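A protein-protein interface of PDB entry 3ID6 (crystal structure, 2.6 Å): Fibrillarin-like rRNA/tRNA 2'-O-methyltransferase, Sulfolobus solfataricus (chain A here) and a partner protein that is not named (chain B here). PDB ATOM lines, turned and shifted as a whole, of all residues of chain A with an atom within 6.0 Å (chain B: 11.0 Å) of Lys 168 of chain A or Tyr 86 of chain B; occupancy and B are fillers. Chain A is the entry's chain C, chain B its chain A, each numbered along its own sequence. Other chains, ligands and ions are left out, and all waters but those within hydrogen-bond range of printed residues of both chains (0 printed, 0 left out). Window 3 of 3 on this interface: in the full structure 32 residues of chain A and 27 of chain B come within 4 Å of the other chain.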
ATOM      1  N   LYS A 141      -4.077   6.390   6.593  1.00  0.00           N
ATOM      2  CA  LYS A 141      -3.912   5.879   7.948  1.00  0.00           C
ATOM      3  C   LYS A 141      -5.155   6.066   8.828  1.00  0.00           C
ATOM      4  O   LYS A 141      -5.424   5.271   9.729  1.00  0.00           O
ATOM      5  CB  LYS A 141      -2.737   6.630   8.568  1.00  0.00           C
ATOM      6  CG  LYS A 141      -2.220   6.082   9.868  1.00  0.00           C
ATOM      7  CD  LYS A 141      -1.384   7.150  10.601  1.00  0.00           C
ATOM      8  CE  LYS A 141      -0.309   6.525  11.505  1.00  0.00           C
ATOM      9  NZ  LYS A 141      -0.882   5.912  12.723  1.00  0.00           N
ATOM     10  N   ALA A 163       6.962   0.016  -0.560  1.00  0.00           N
ATOM     11  CA  ALA A 163       6.339  -1.160   0.011  1.00  0.00           C
ATOM     12  C   ALA A 163       6.755  -1.328   1.473  1.00  0.00           C
ATOM     13  O   ALA A 163       5.916  -1.598   2.338  1.00  0.00           O
ATOM     14  CB  ALA A 163       6.710  -2.379  -0.795  1.00  0.00           C
ATOM     15  N   ILE A 164       8.046  -1.143   1.739  1.00  0.00           N
ATOM     16  CA  ILE A 164       8.596  -1.269   3.095  1.00  0.00           C
ATOM     17  C   ILE A 164       8.008  -0.223   4.056  1.00  0.00           C
ATOM     18  O   ILE A 164       7.640  -0.543   5.194  1.00  0.00           O
ATOM     19  CB  ILE A 164      10.152  -1.220   3.082  1.00  0.00           C
ATOM     20  CG1 ILE A 164      10.715  -2.553   2.568  1.00  0.00           C
ATOM     21  CG2 ILE A 164      10.711  -0.884   4.467  1.00  0.00           C
ATOM     22  CD1 ILE A 164      12.146  -2.480   2.033  1.00  0.00           C
ATOM     23  N   TYR A 165       7.921   1.018   3.586  1.00  0.00           N
ATOM     24  CA  TYR A 165       7.350   2.100   4.369  1.00  0.00           C
ATOM     25  C   TYR A 165       5.902   1.756   4.756  1.00  0.00           C
ATOM     26  O   TYR A 165       5.517   1.900   5.915  1.00  0.00           O
ATOM     27  CB  TYR A 165       7.434   3.408   3.578  1.00  0.00           C
ATOM     28  CG  TYR A 165       7.227   4.685   4.373  1.00  0.00           C
ATOM     29  CD1 TYR A 165       7.791   4.851   5.644  1.00  0.00           C
ATOM     30  CD2 TYR A 165       6.499   5.751   3.828  1.00  0.00           C
ATOM     31  CE1 TYR A 165       7.613   6.045   6.364  1.00  0.00           C
ATOM     32  CE2 TYR A 165       6.315   6.937   4.530  1.00  0.00           C
ATOM     33  CZ  TYR A 165       6.873   7.079   5.797  1.00  0.00           C
ATOM     34  OH  TYR A 165       6.687   8.254   6.490  1.00  0.00           O
ATOM     35  N   ASN A 166       5.126   1.267   3.793  1.00  0.00           N
ATOM     36  CA  ASN A 166       3.758   0.823   4.049  1.00  0.00           C
ATOM     37  C   ASN A 166       3.666  -0.345   5.026  1.00  0.00           C
ATOM     38  O   ASN A 166       2.814  -0.356   5.923  1.00  0.00           O
ATOM     39  CB  ASN A 166       3.045   0.481   2.743  1.00  0.00           C
ATOM     40  CG  ASN A 166       2.379   1.681   2.133  1.00  0.00           C
ATOM     41  OD1 ASN A 166       1.206   1.929   2.384  1.00  0.00           O
ATOM     42  ND2 ASN A 166       3.131   2.460   1.359  1.00  0.00           N
ATOM     43  N   ALA A 167       4.566  -1.308   4.853  1.00  0.00           N
ATOM     44  CA  ALA A 167       4.636  -2.464   5.726  1.00  0.00           C
ATOM     45  C   ALA A 167       4.748  -2.057   7.197  1.00  0.00           C
ATOM     46  O   ALA A 167       3.965  -2.526   8.027  1.00  0.00           O
ATOM     47  CB  ALA A 167       5.791  -3.367   5.323  1.00  0.00           C
ATOM     48  N   LYS A 168       5.687  -1.173   7.523  1.00  0.00           N
ATOM     49  CA  LYS A 168       5.863  -0.788   8.925  1.00  0.00           C
ATOM     50  C   LYS A 168       4.681  -0.021   9.536  1.00  0.00           C
ATOM     51  O   LYS A 168       4.528   0.002  10.751  1.00  0.00           O
ATOM     52  CB  LYS A 168       7.216  -0.099   9.195  1.00  0.00           C
ATOM     53  CG  LYS A 168       7.656   0.951   8.185  1.00  0.00           C
ATOM     54  CD  LYS A 168       9.107   1.381   8.411  1.00  0.00           C
ATOM     55  CE  LYS A 168      10.100   0.290   8.056  1.00  0.00           C
ATOM     56  NZ  LYS A 168      11.423   0.849   7.612  1.00  0.00           N
ATOM     57  N   PHE A 169       3.843   0.579   8.693  1.00  0.00           N
ATOM     58  CA  PHE A 169       2.584   1.159   9.140  1.00  0.00           C
ATOM     59  C   PHE A 169       1.522   0.086   9.365  1.00  0.00           C
ATOM     60  O   PHE A 169       0.898   0.045  10.424  1.00  0.00           O
ATOM     61  CB  PHE A 169       2.043   2.132   8.096  1.00  0.00           C
ATOM     62  CG  PHE A 169       2.554   3.524   8.226  1.00  0.00           C
ATOM     63  CD1 PHE A 169       3.688   3.922   7.540  1.00  0.00           C
ATOM     64  CD2 PHE A 169       1.871   4.456   9.011  1.00  0.00           C
ATOM     65  CE1 PHE A 169       4.164   5.229   7.650  1.00  0.00           C
ATOM     66  CE2 PHE A 169       2.320   5.767   9.127  1.00  0.00           C
ATOM     67  CZ  PHE A 169       3.474   6.160   8.450  1.00  0.00           C
ATOM     68  N   PHE A 170       1.338  -0.785   8.370  1.00  0.00           N
ATOM     69  CA  PHE A 170       0.106  -1.579   8.240  1.00  0.00           C
ATOM     70  C   PHE A 170       0.190  -3.099   8.380  1.00  0.00           C
ATOM     71  O   PHE A 170      -0.795  -3.730   8.769  1.00  0.00           O
ATOM     72  CB  PHE A 170      -0.602  -1.241   6.925  1.00  0.00           C
ATOM     73  CG  PHE A 170      -0.960   0.203   6.798  1.00  0.00           C
ATOM     74  CD1 PHE A 170      -0.432   0.971   5.771  1.00  0.00           C
ATOM     75  CD2 PHE A 170      -1.802   0.807   7.733  1.00  0.00           C
ATOM     76  CE1 PHE A 170      -0.753   2.316   5.659  1.00  0.00           C
ATOM     77  CE2 PHE A 170      -2.118   2.151   7.639  1.00  0.00           C
ATOM     78  CZ  PHE A 170      -1.602   2.909   6.598  1.00  0.00           C
ATOM     79  N   LEU A 171       1.334  -3.687   8.034  1.00  0.00           N
ATOM     80  CA  LEU A 171       1.440  -5.136   7.960  1.00  0.00           C
ATOM     81  C   LEU A 171       1.614  -5.722   9.349  1.00  0.00           C
ATOM     82  O   LEU A 171       2.510  -5.319  10.093  1.00  0.00           O
ATOM     83  CB  LEU A 171       2.625  -5.541   7.079  1.00  0.00           C
ATOM     84  CG  LEU A 171       2.452  -6.508   5.897  1.00  0.00           C
ATOM     85  CD1 LEU A 171       3.753  -7.237   5.616  1.00  0.00           C
ATOM     86  CD2 LEU A 171       1.303  -7.510   6.064  1.00  0.00           C
ATOM     87  N   ASN A 207      15.038  -6.279   6.906  1.00  0.00           N
ATOM     88  CA  ASN A 207      13.884  -6.459   7.816  1.00  0.00           C
ATOM     89  C   ASN A 207      12.836  -7.526   7.393  1.00  0.00           C
ATOM     90  O   ASN A 207      11.985  -7.911   8.196  1.00  0.00           O
ATOM     91  CB  ASN A 207      13.192  -5.122   8.115  1.00  0.00           C
ATOM     92  CG  ASN A 207      13.261  -4.137   6.953  1.00  0.00           C
ATOM     93  OD1 ASN A 207      13.877  -4.397   5.924  1.00  0.00           O
ATOM     94  ND2 ASN A 207      12.630  -2.987   7.128  1.00  0.00           N
ATOM     95  N   TYR A 230       7.257 -10.593   6.816  1.00  0.00           N
ATOM     96  CA  TYR A 230       7.685  -9.534   7.719  1.00  0.00           C
ATOM     97  C   TYR A 230       7.985 -10.151   9.083  1.00  0.00           C
ATOM     98  O   TYR A 230       7.127 -10.801   9.680  1.00  0.00           O
ATOM     99  CB  TYR A 230       6.602  -8.451   7.806  1.00  0.00           C
ATOM    100  CG  TYR A 230       6.981  -7.198   8.568  1.00  0.00           C
ATOM    101  CD1 TYR A 230       8.122  -6.461   8.236  1.00  0.00           C
ATOM    102  CD2 TYR A 230       6.180  -6.732   9.612  1.00  0.00           C
ATOM    103  CE1 TYR A 230       8.465  -5.294   8.942  1.00  0.00           C
ATOM    104  CE2 TYR A 230       6.517  -5.570  10.321  1.00  0.00           C
ATOM    105  CZ  TYR A 230       7.655  -4.859   9.979  1.00  0.00           C
ATOM    106  OH  TYR A 230       7.974  -3.720  10.682  1.00  0.00           O
ATOM    107  N   TYR B   5      -0.041   9.547  23.140  1.00  0.00           N
ATOM    108  CA  TYR B   5      -0.023   9.290  21.696  1.00  0.00           C
ATOM    109  C   TYR B   5      -1.385   9.601  21.110  1.00  0.00           C
ATOM    110  O   TYR B   5      -2.382   9.002  21.515  1.00  0.00           O
ATOM    111  CB  TYR B   5       0.337   7.832  21.417  1.00  0.00           C
ATOM    112  CG  TYR B   5       1.793   7.517  21.638  1.00  0.00           C
ATOM    113  CD1 TYR B   5       2.680   7.466  20.566  1.00  0.00           C
ATOM    114  CD2 TYR B   5       2.289   7.269  22.923  1.00  0.00           C
ATOM    115  CE1 TYR B   5       4.029   7.173  20.763  1.00  0.00           C
ATOM    116  CE2 TYR B   5       3.634   6.978  23.132  1.00  0.00           C
ATOM    117  CZ  TYR B   5       4.500   6.934  22.050  1.00  0.00           C
ATOM    118  OH  TYR B   5       5.834   6.648  22.251  1.00  0.00           O
ATOM    119  N   LEU B   6      -1.432  10.541  20.170  1.00  0.00           N
ATOM    120  CA  LEU B   6      -2.693  10.908  19.532  1.00  0.00           C
ATOM    121  C   LEU B   6      -3.017   9.990  18.358  1.00  0.00           C
ATOM    122  O   LEU B   6      -2.255   9.906  17.385  1.00  0.00           O
ATOM    123  CB  LEU B   6      -2.669  12.358  19.056  1.00  0.00           C
ATOM    124  CG  LEU B   6      -3.953  13.210  19.085  1.00  0.00           C
ATOM    125  CD1 LEU B   6      -4.009  14.059  17.830  1.00  0.00           C
ATOM    126  CD2 LEU B   6      -5.245  12.399  19.224  1.00  0.00           C
ATOM    127  N   ILE B   7      -4.148   9.300  18.462  1.00  0.00           N
ATOM    128  CA  ILE B   7      -4.687   8.526  17.345  1.00  0.00           C
ATOM    129  C   ILE B   7      -5.934   9.239  16.817  1.00  0.00           C
ATOM    130  O   ILE B   7      -6.822   9.615  17.591  1.00  0.00           O
ATOM    131  CB  ILE B   7      -4.956   7.043  17.744  1.00  0.00           C
ATOM    132  CG1 ILE B   7      -3.733   6.167  17.442  1.00  0.00           C
ATOM    133  CG2 ILE B   7      -6.139   6.477  16.993  1.00  0.00           C
ATOM    134  CD1 ILE B   7      -2.568   6.285  18.453  1.00  0.00           C
ATOM    135  N   VAL B  64       2.338  12.970  21.205  1.00  0.00           N
ATOM    136  CA  VAL B  64       2.966  12.514  19.968  1.00  0.00           C
ATOM    137  C   VAL B  64       1.913  12.181  18.909  1.00  0.00           C
ATOM    138  O   VAL B  64       0.852  11.626  19.211  1.00  0.00           O
ATOM    139  CB  VAL B  64       4.066  11.410  20.163  1.00  0.00           C
ATOM    140  CG1 VAL B  64       3.988  10.751  21.536  1.00  0.00           C
ATOM    141  CG2 VAL B  64       4.053  10.387  19.016  1.00  0.00           C
ATOM    142  N   VAL B  65       2.222  12.562  17.673  1.00  0.00           N
ATOM    143  CA  VAL B  65       1.262  12.559  16.581  1.00  0.00           C
ATOM    144  C   VAL B  65       1.758  11.713  15.401  1.00  0.00           C
ATOM    145  O   VAL B  65       2.949  11.412  15.285  1.00  0.00           O
ATOM    146  CB  VAL B  65       0.934  14.013  16.134  1.00  0.00           C
ATOM    147  CG1 VAL B  65      -0.181  14.028  15.119  1.00  0.00           C
ATOM    148  CG2 VAL B  65       0.526  14.853  17.323  1.00  0.00           C
ATOM    149  N   GLU B  66       0.816  11.333  14.540  1.00  0.00           N
ATOM    150  CA  GLU B  66       1.051  10.472  13.379  1.00  0.00           C
ATOM    151  C   GLU B  66       1.432  11.254  12.100  1.00  0.00           C
ATOM    152  O   GLU B  66       2.091  10.707  11.212  1.00  0.00           O
ATOM    153  CB  GLU B  66      -0.203   9.626  13.122  1.00  0.00           C
ATOM    154  CG  GLU B  66      -0.773   8.931  14.369  1.00  0.00           C
ATOM    155  CD  GLU B  66      -2.246   8.498  14.230  1.00  0.00           C
ATOM    156  OE1 GLU B  66      -3.135   9.337  13.907  1.00  0.00           O
ATOM    157  OE2 GLU B  66      -2.516   7.303  14.476  1.00  0.00           O
ATOM    158  N   ASN B  67       1.019  12.520  12.012  1.00  0.00           N
ATOM    159  CA  ASN B  67       1.275  13.353  10.823  1.00  0.00           C
ATOM    160  C   ASN B  67       2.010  14.649  11.175  1.00  0.00           C
ATOM    161  O   ASN B  67       1.490  15.486  11.914  1.00  0.00           O
ATOM    162  CB  ASN B  67      -0.041  13.656  10.076  1.00  0.00           C
ATOM    163  CG  ASN B  67       0.182  14.338   8.721  1.00  0.00           C
ATOM    164  OD1 ASN B  67       0.992  13.893   7.901  1.00  0.00           O
ATOM    165  ND2 ASN B  67      -0.556  15.417   8.481  1.00  0.00           N
ATOM    166  N   GLU B  68       3.212  14.811  10.621  1.00  0.00           N
ATOM    167  CA  GLU B  68       4.110  15.914  10.997  1.00  0.00           C
ATOM    168  C   GLU B  68       3.694  17.321  10.534  1.00  0.00           C
ATOM    169  O   GLU B  68       4.359  18.307  10.865  1.00  0.00           O
ATOM    170  CB  GLU B  68       5.574  15.603  10.628  1.00  0.00           C
ATOM    171  CG  GLU B  68       5.867  15.455   9.140  1.00  0.00           C
ATOM    172  CD  GLU B  68       7.356  15.325   8.835  1.00  0.00           C
ATOM    173  OE1 GLU B  68       8.191  15.735   9.676  1.00  0.00           O
ATOM    174  OE2 GLU B  68       7.688  14.816   7.742  1.00  0.00           O
ATOM    175  N   SER B  82       5.441  16.224  19.442  1.00  0.00           N
ATOM    176  CA  SER B  82       6.445  15.558  18.616  1.00  0.00           C
ATOM    177  C   SER B  82       5.842  14.549  17.628  1.00  0.00           C
ATOM    178  O   SER B  82       4.666  14.175  17.715  1.00  0.00           O
ATOM    179  CB  SER B  82       7.549  14.919  19.472  1.00  0.00           C
ATOM    180  OG  SER B  82       7.082  13.781  20.168  1.00  0.00           O
ATOM    181  N   TYR B  83       6.674  14.123  16.684  1.00  0.00           N
ATOM    182  CA  TYR B  83       6.249  13.247  15.612  1.00  0.00           C
ATOM    183  C   TYR B  83       6.930  11.886  15.715  1.00  0.00           C
ATOM    184  O   TYR B  83       8.161  11.793  15.803  1.00  0.00           O
ATOM    185  CB  TYR B  83       6.543  13.912  14.261  1.00  0.00           C
ATOM    186  CG  TYR B  83       6.304  13.034  13.058  1.00  0.00           C
ATOM    187  CD1 TYR B  83       5.018  12.598  12.736  1.00  0.00           C
ATOM    188  CD2 TYR B  83       7.361  12.654  12.227  1.00  0.00           C
ATOM    189  CE1 TYR B  83       4.787  11.792  11.629  1.00  0.00           C
ATOM    190  CE2 TYR B  83       7.144  11.844  11.108  1.00  0.00           C
ATOM    191  CZ  TYR B  83       5.851  11.419  10.820  1.00  0.00           C
ATOM    192  OH  TYR B  83       5.612  10.617   9.728  1.00  0.00           O
ATOM    193  N   GLU B  84       6.110  10.839  15.737  1.00  0.00           N
ATOM    194  CA  GLU B  84       6.598   9.475  15.577  1.00  0.00           C
ATOM    195  C   GLU B  84       5.857   8.815  14.416  1.00  0.00           C
ATOM    196  O   GLU B  84       4.634   8.615  14.481  1.00  0.00           O
ATOM    197  CB  GLU B  84       6.513   8.673  16.877  1.00  0.00           C
ATOM    198  CG  GLU B  84       7.673   8.995  17.830  1.00  0.00           C
ATOM    199  CD  GLU B  84       7.452   8.510  19.253  1.00  0.00           C
ATOM    200  OE1 GLU B  84       7.016   7.347  19.426  1.00  0.00           O
ATOM    201  OE2 GLU B  84       7.733   9.290  20.197  1.00  0.00           O
ATOM    202  N   PRO B  85       6.603   8.506  13.336  1.00  0.00           N
ATOM    203  CA  PRO B  85       6.031   8.052  12.075  1.00  0.00           C
ATOM    204  C   PRO B  85       5.115   6.834  12.233  1.00  0.00           C
ATOM    205  O   PRO B  85       3.882   6.967  12.114  1.00  0.00           O
ATOM    206  CB  PRO B  85       7.266   7.709  11.223  1.00  0.00           C
ATOM    207  CG  PRO B  85       8.380   8.488  11.819  1.00  0.00           C
ATOM    208  CD  PRO B  85       8.077   8.575  13.284  1.00  0.00           C
ATOM    209  N   TYR B  86       5.706   5.674  12.511  1.00  0.00           N
ATOM    210  CA  TYR B  86       4.963   4.409  12.526  1.00  0.00           C
ATOM    211  C   TYR B  86       5.119   3.721  13.880  1.00  0.00           C
ATOM    212  O   TYR B  86       5.707   2.631  13.978  1.00  0.00           O
ATOM    213  CB  TYR B  86       5.444   3.504  11.387  1.00  0.00           C
ATOM    214  CG  TYR B  86       6.901   3.725  11.022  1.00  0.00           C
ATOM    215  CD1 TYR B  86       7.934   3.229  11.831  1.00  0.00           C
ATOM    216  CD2 TYR B  86       7.251   4.441   9.877  1.00  0.00           C
ATOM    217  CE1 TYR B  86       9.275   3.439  11.505  1.00  0.00           C
ATOM    218  CE2 TYR B  86       8.596   4.660   9.543  1.00  0.00           C
ATOM    219  CZ  TYR B  86       9.598   4.157  10.361  1.00  0.00           C
ATOM    220  OH  TYR B  86      10.922   4.359  10.026  1.00  0.00           O
ATOM    221  N   SER B  87       4.594   4.374  14.919  1.00  0.00           N
ATOM    222  CA  SER B  87       4.795   3.933  16.295  1.00  0.00           C
ATOM    223  C   SER B  87       4.054   2.631  16.620  1.00  0.00           C
ATOM    224  O   SER B  87       3.003   2.350  16.045  1.00  0.00           O
ATOM    225  CB  SER B  87       4.393   5.039  17.280  1.00  0.00           C
ATOM    226  OG  SER B  87       3.002   5.304  17.222  1.00  0.00           O
ATOM    227  N   LYS B  88       4.634   1.851  17.534  1.00  0.00           N
ATOM    228  CA  LYS B  88       4.029   0.637  18.084  1.00  0.00           C
ATOM    229  C   LYS B  88       2.596   0.855  18.547  1.00  0.00           C
ATOM    230  O   LYS B  88       1.727   0.026  18.276  1.00  0.00           O
ATOM    231  CB  LYS B  88       4.854   0.119  19.264  1.00  0.00           C
ATOM    232  CG  LYS B  88       6.259  -0.327  18.885  1.00  0.00           C
ATOM    233  CD  LYS B  88       7.181  -0.398  20.098  1.00  0.00           C
ATOM    234  CE  LYS B  88       8.561  -0.913  19.703  1.00  0.00           C
ATOM    235  NZ  LYS B  88       9.494  -0.944  20.867  1.00  0.00           N
ATOM    236  N   VAL B  89       2.362   1.974  19.234  1.00  0.00           N
ATOM    237  CA  VAL B  89       1.041   2.320  19.783  1.00  0.00           C
ATOM    238  C   VAL B  89      -0.031   2.505  18.693  1.00  0.00           C
ATOM    239  O   VAL B  89      -1.182   2.088  18.868  1.00  0.00           O
ATOM    240  CB  VAL B  89       1.104   3.570  20.717  1.00  0.00           C
ATOM    241  CG1 VAL B  89      -0.284   4.128  20.987  1.00  0.00           C
ATOM    242  CG2 VAL B  89       1.816   3.239  22.033  1.00  0.00           C
ATOM    243  N   SER B  90       0.340   3.118  17.577  1.00  0.00           N
ATOM    244  CA  SER B  90      -0.624   3.313  16.502  1.00  0.00           C
ATOM    245  C   SER B  90      -0.908   1.978  15.788  1.00  0.00           C
ATOM    246  O   SER B  90      -2.050   1.685  15.400  1.00  0.00           O
ATOM    247  CB  SER B  90      -0.165   4.406  15.542  1.00  0.00           C
ATOM    248  OG  SER B  90       0.925   3.958  14.765  1.00  0.00           O
ATOM    249  N   ARG B  91       0.127   1.159  15.652  1.00  0.00           N
ATOM    250  CA  ARG B  91      -0.059  -0.203  15.187  1.00  0.00           C
ATOM    251  C   ARG B  91      -1.009  -0.981  16.120  1.00  0.00           C
ATOM    252  O   ARG B  91      -1.925  -1.649  15.639  1.00  0.00           O
ATOM    253  CB  ARG B  91       1.286  -0.898  15.030  1.00  0.00           C
ATOM    254  CG  ARG B  91       2.111  -0.359  13.870  1.00  0.00           C
ATOM    255  CD  ARG B  91       3.477  -1.011  13.808  1.00  0.00           C
ATOM    256  NE  ARG B  91       3.393  -2.471  13.746  1.00  0.00           N
ATOM    257  CZ  ARG B  91       3.233  -3.175  12.625  1.00  0.00           C
ATOM    258  NH1 ARG B  91       3.145  -2.556  11.449  1.00  0.00           N
ATOM    259  NH2 ARG B  91       3.178  -4.502  12.676  1.00  0.00           N
ATOM    260  N   ILE B  92      -0.809  -0.852  17.439  1.00  0.00           N
ATOM    261  CA  ILE B  92      -1.660  -1.497  18.452  1.00  0.00           C
ATOM    262  C   ILE B  92      -3.121  -1.044  18.351  1.00  0.00           C
ATOM    263  O   ILE B  92      -4.052  -1.824  18.592  1.00  0.00           O
ATOM    264  CB  ILE B  92      -1.131  -1.243  19.892  1.00  0.00           C
ATOM    265  CG1 ILE B  92       0.122  -2.089  20.153  1.00  0.00           C
ATOM    266  CG2 ILE B  92      -2.227  -1.524  20.944  1.00  0.00           C
ATOM    267  CD1 ILE B  92       0.938  -1.670  21.379  1.00  0.00           C
ATOM    268  N   PHE B  93      -3.314   0.222  18.003  1.00  0.00           N
ATOM    269  CA  PHE B  93      -4.638   0.707  17.712  1.00  0.00           C
ATOM    270  C   PHE B  93      -5.254   0.007  16.489  1.00  0.00           C
ATOM    271  O   PHE B  93      -6.422  -0.386  16.523  1.00  0.00           O
ATOM    272  CB  PHE B  93      -4.634   2.220  17.516  1.00  0.00           C
ATOM    273  CG  PHE B  93      -5.876   2.727  16.863  1.00  0.00           C
ATOM    274  CD1 PHE B  93      -7.080   2.751  17.562  1.00  0.00           C
ATOM    275  CD2 PHE B  93      -5.860   3.119  15.539  1.00  0.00           C
ATOM    276  CE1 PHE B  93      -8.248   3.199  16.957  1.00  0.00           C
ATOM    277  CE2 PHE B  93      -7.018   3.574  14.921  1.00  0.00           C
ATOM    278  CZ  PHE B  93      -8.216   3.613  15.631  1.00  0.00           C
ATOM    279  N   ARG B  94      -4.487  -0.146  15.412  1.00  0.00           N
ATOM    280  CA  ARG B  94      -5.035  -0.746  14.190  1.00  0.00           C
ATOM    281  C   ARG B  94      -5.263  -2.264  14.288  1.00  0.00           C
ATOM    282  O   ARG B  94      -6.146  -2.809  13.607  1.00  0.00           O
ATOM    283  CB  ARG B  94      -4.206  -0.367  12.954  1.00  0.00           C
ATOM    284  CG  ARG B  94      -4.377   1.087  12.530  1.00  0.00           C
ATOM    285  CD  ARG B  94      -3.655   1.420  11.221  1.00  0.00           C
ATOM    286  NE  ARG B  94      -2.201   1.298  11.330  1.00  0.00           N
ATOM    287  CZ  ARG B  94      -1.388   2.267  11.738  1.00  0.00           C
ATOM    288  NH1 ARG B  94      -0.082   2.056  11.818  1.00  0.00           N
ATOM    289  NH2 ARG B  94      -1.879   3.446  12.080  1.00  0.00           N
ATOM    290  N   GLU B  95      -4.482  -2.935  15.140  1.00  0.00           N
ATOM    291  CA  GLU B  95      -4.630  -4.377  15.377  1.00  0.00           C
ATOM    292  C   GLU B  95      -5.967  -4.683  16.050  1.00  0.00           C
ATOM    293  O   GLU B  95      -6.495  -5.783  15.920  1.00  0.00           O
ATOM    294  CB  GLU B  95      -3.518  -4.917  16.285  1.00  0.00           C
ATOM    295  CG  GLU B  95      -2.084  -4.514  15.938  1.00  0.00           C
ATOM    296  CD  GLU B  95      -1.483  -5.302  14.784  1.00  0.00           C
ATOM    297  OE1 GLU B  95      -2.067  -6.337  14.380  1.00  0.00           O
ATOM    298  OE2 GLU B  95      -0.410  -4.884  14.285  1.00  0.00           O
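The side-chain amino group (NZ) of Lys 141 of chain A lies within salt-bridge range of the side-chain carboxylate (OE2) of Glu 66 of chain B, 2.8 Å away. The side-chain hydroxyl of Ser 90 of chain B lies close to the side-chain amino group of Lys 141 of chain A (3.4 Å). The guanidinium group of Arg 91 of chain B lies within hydrogen-bond range of the backbone carbonyl oxygen of Lys 168 of chain A (3.0 Å). O of Leu 171 of chain A is in hydrogen-bond range of NH2 of Arg 91 of chain B, at 2.8 Å. The side-chain amino group (NZ) of Lys 141 of chain A sits close to the guanidinium group (NH2) of Arg 94 of chain B, at 2.7 Å. NH1 of Arg 94 of chain B lies within hydrogen-bond range of O of Phe 169 of chain A, at 2.6 Å.
O of Ser 87 of chain B lies within hydrogen-bond range of OG of Ser 90 of chain B, at 2.9 Å. NH2 of Arg 91 of chain B is in salt-bridge range of OE2 of Glu 95 of chain B, 3.95 Å away.
Among the printed residues, merely in contact across the chains: Tyr 165 of chain A with Tyr 86 of chain B (3.6 Å), Ala 167 of chain A with Arg 91 of chain B (3.5 Å), Lys 168 of chain A with Tyr 86 of chain B (3.4 Å), Phe 169 of chain A with Pro 85 of chain B (3.6 Å), Phe 169 of chain A with Tyr 86 of chain B (3.9 Å), Phe 169 of chain A with Arg 91 of chain B (3.6 Å), Phe 170 of chain A with Arg 91 of chain B (3.99 Å) and Phe 170 of chain A with Arg 94 of chain B (3.7 Å).
Lys 168 of chain A touches just these residues of chain B: Tyr 86 and Arg 91. Tyr 86 of chain B touches just these residues of chain A: Tyr 165, Lys 168 and Phe 169. No residue of chain B comes within 4 Å of Ile 164 of chain A. Of chain B, only Arg 91 (3.5 Å) comes within 4 Å of Ala 167 of chain A. Phe 169 of chain A touches just these residues of chain B: Pro 85 (3.6 Å), Tyr 86 (3.9 Å), Arg 91 (3.6 Å) and Arg 94 (2.6 Å). Printed residues of chain A within 4 Å of Ser 90 of chain B: Lys 141. Of the printed residues of chain A, Arg 94 of chain B touches Lys 141, Phe 169 and Phe 170. Printed residues of chain A within 4 Å of Arg 91 of chain B: Ala 167, Lys 168, Phe 169, Phe 170 and Leu 171. Of the printed residues of chain A, Glu 66 of chain B touches Lys 141 (2.8 Å). Of the printed residues of chain B, Lys 141 of chain A touches Glu 66, Ser 90 and Arg 94. Ser 87 of chain B touches none of the printed residues of chain A. The nearest residue of chain A that does not touch Tyr 86 of chain B is Lys 141 of chain A (5.8 Å). The nearest printed residue of chain B that does not touch Leu 171 of chain A is Glu 95 of chain B (5.1 Å).
Hydrophobic or aromatic side chains of chain A that line the printed part of chain B: Tyr 165, Phe 169 and Phe 170. Along chain A the printed residues that touch a printed residue of chain B span positions 141 to 171. Among the printed residues, 14 pairs touch across the chains.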
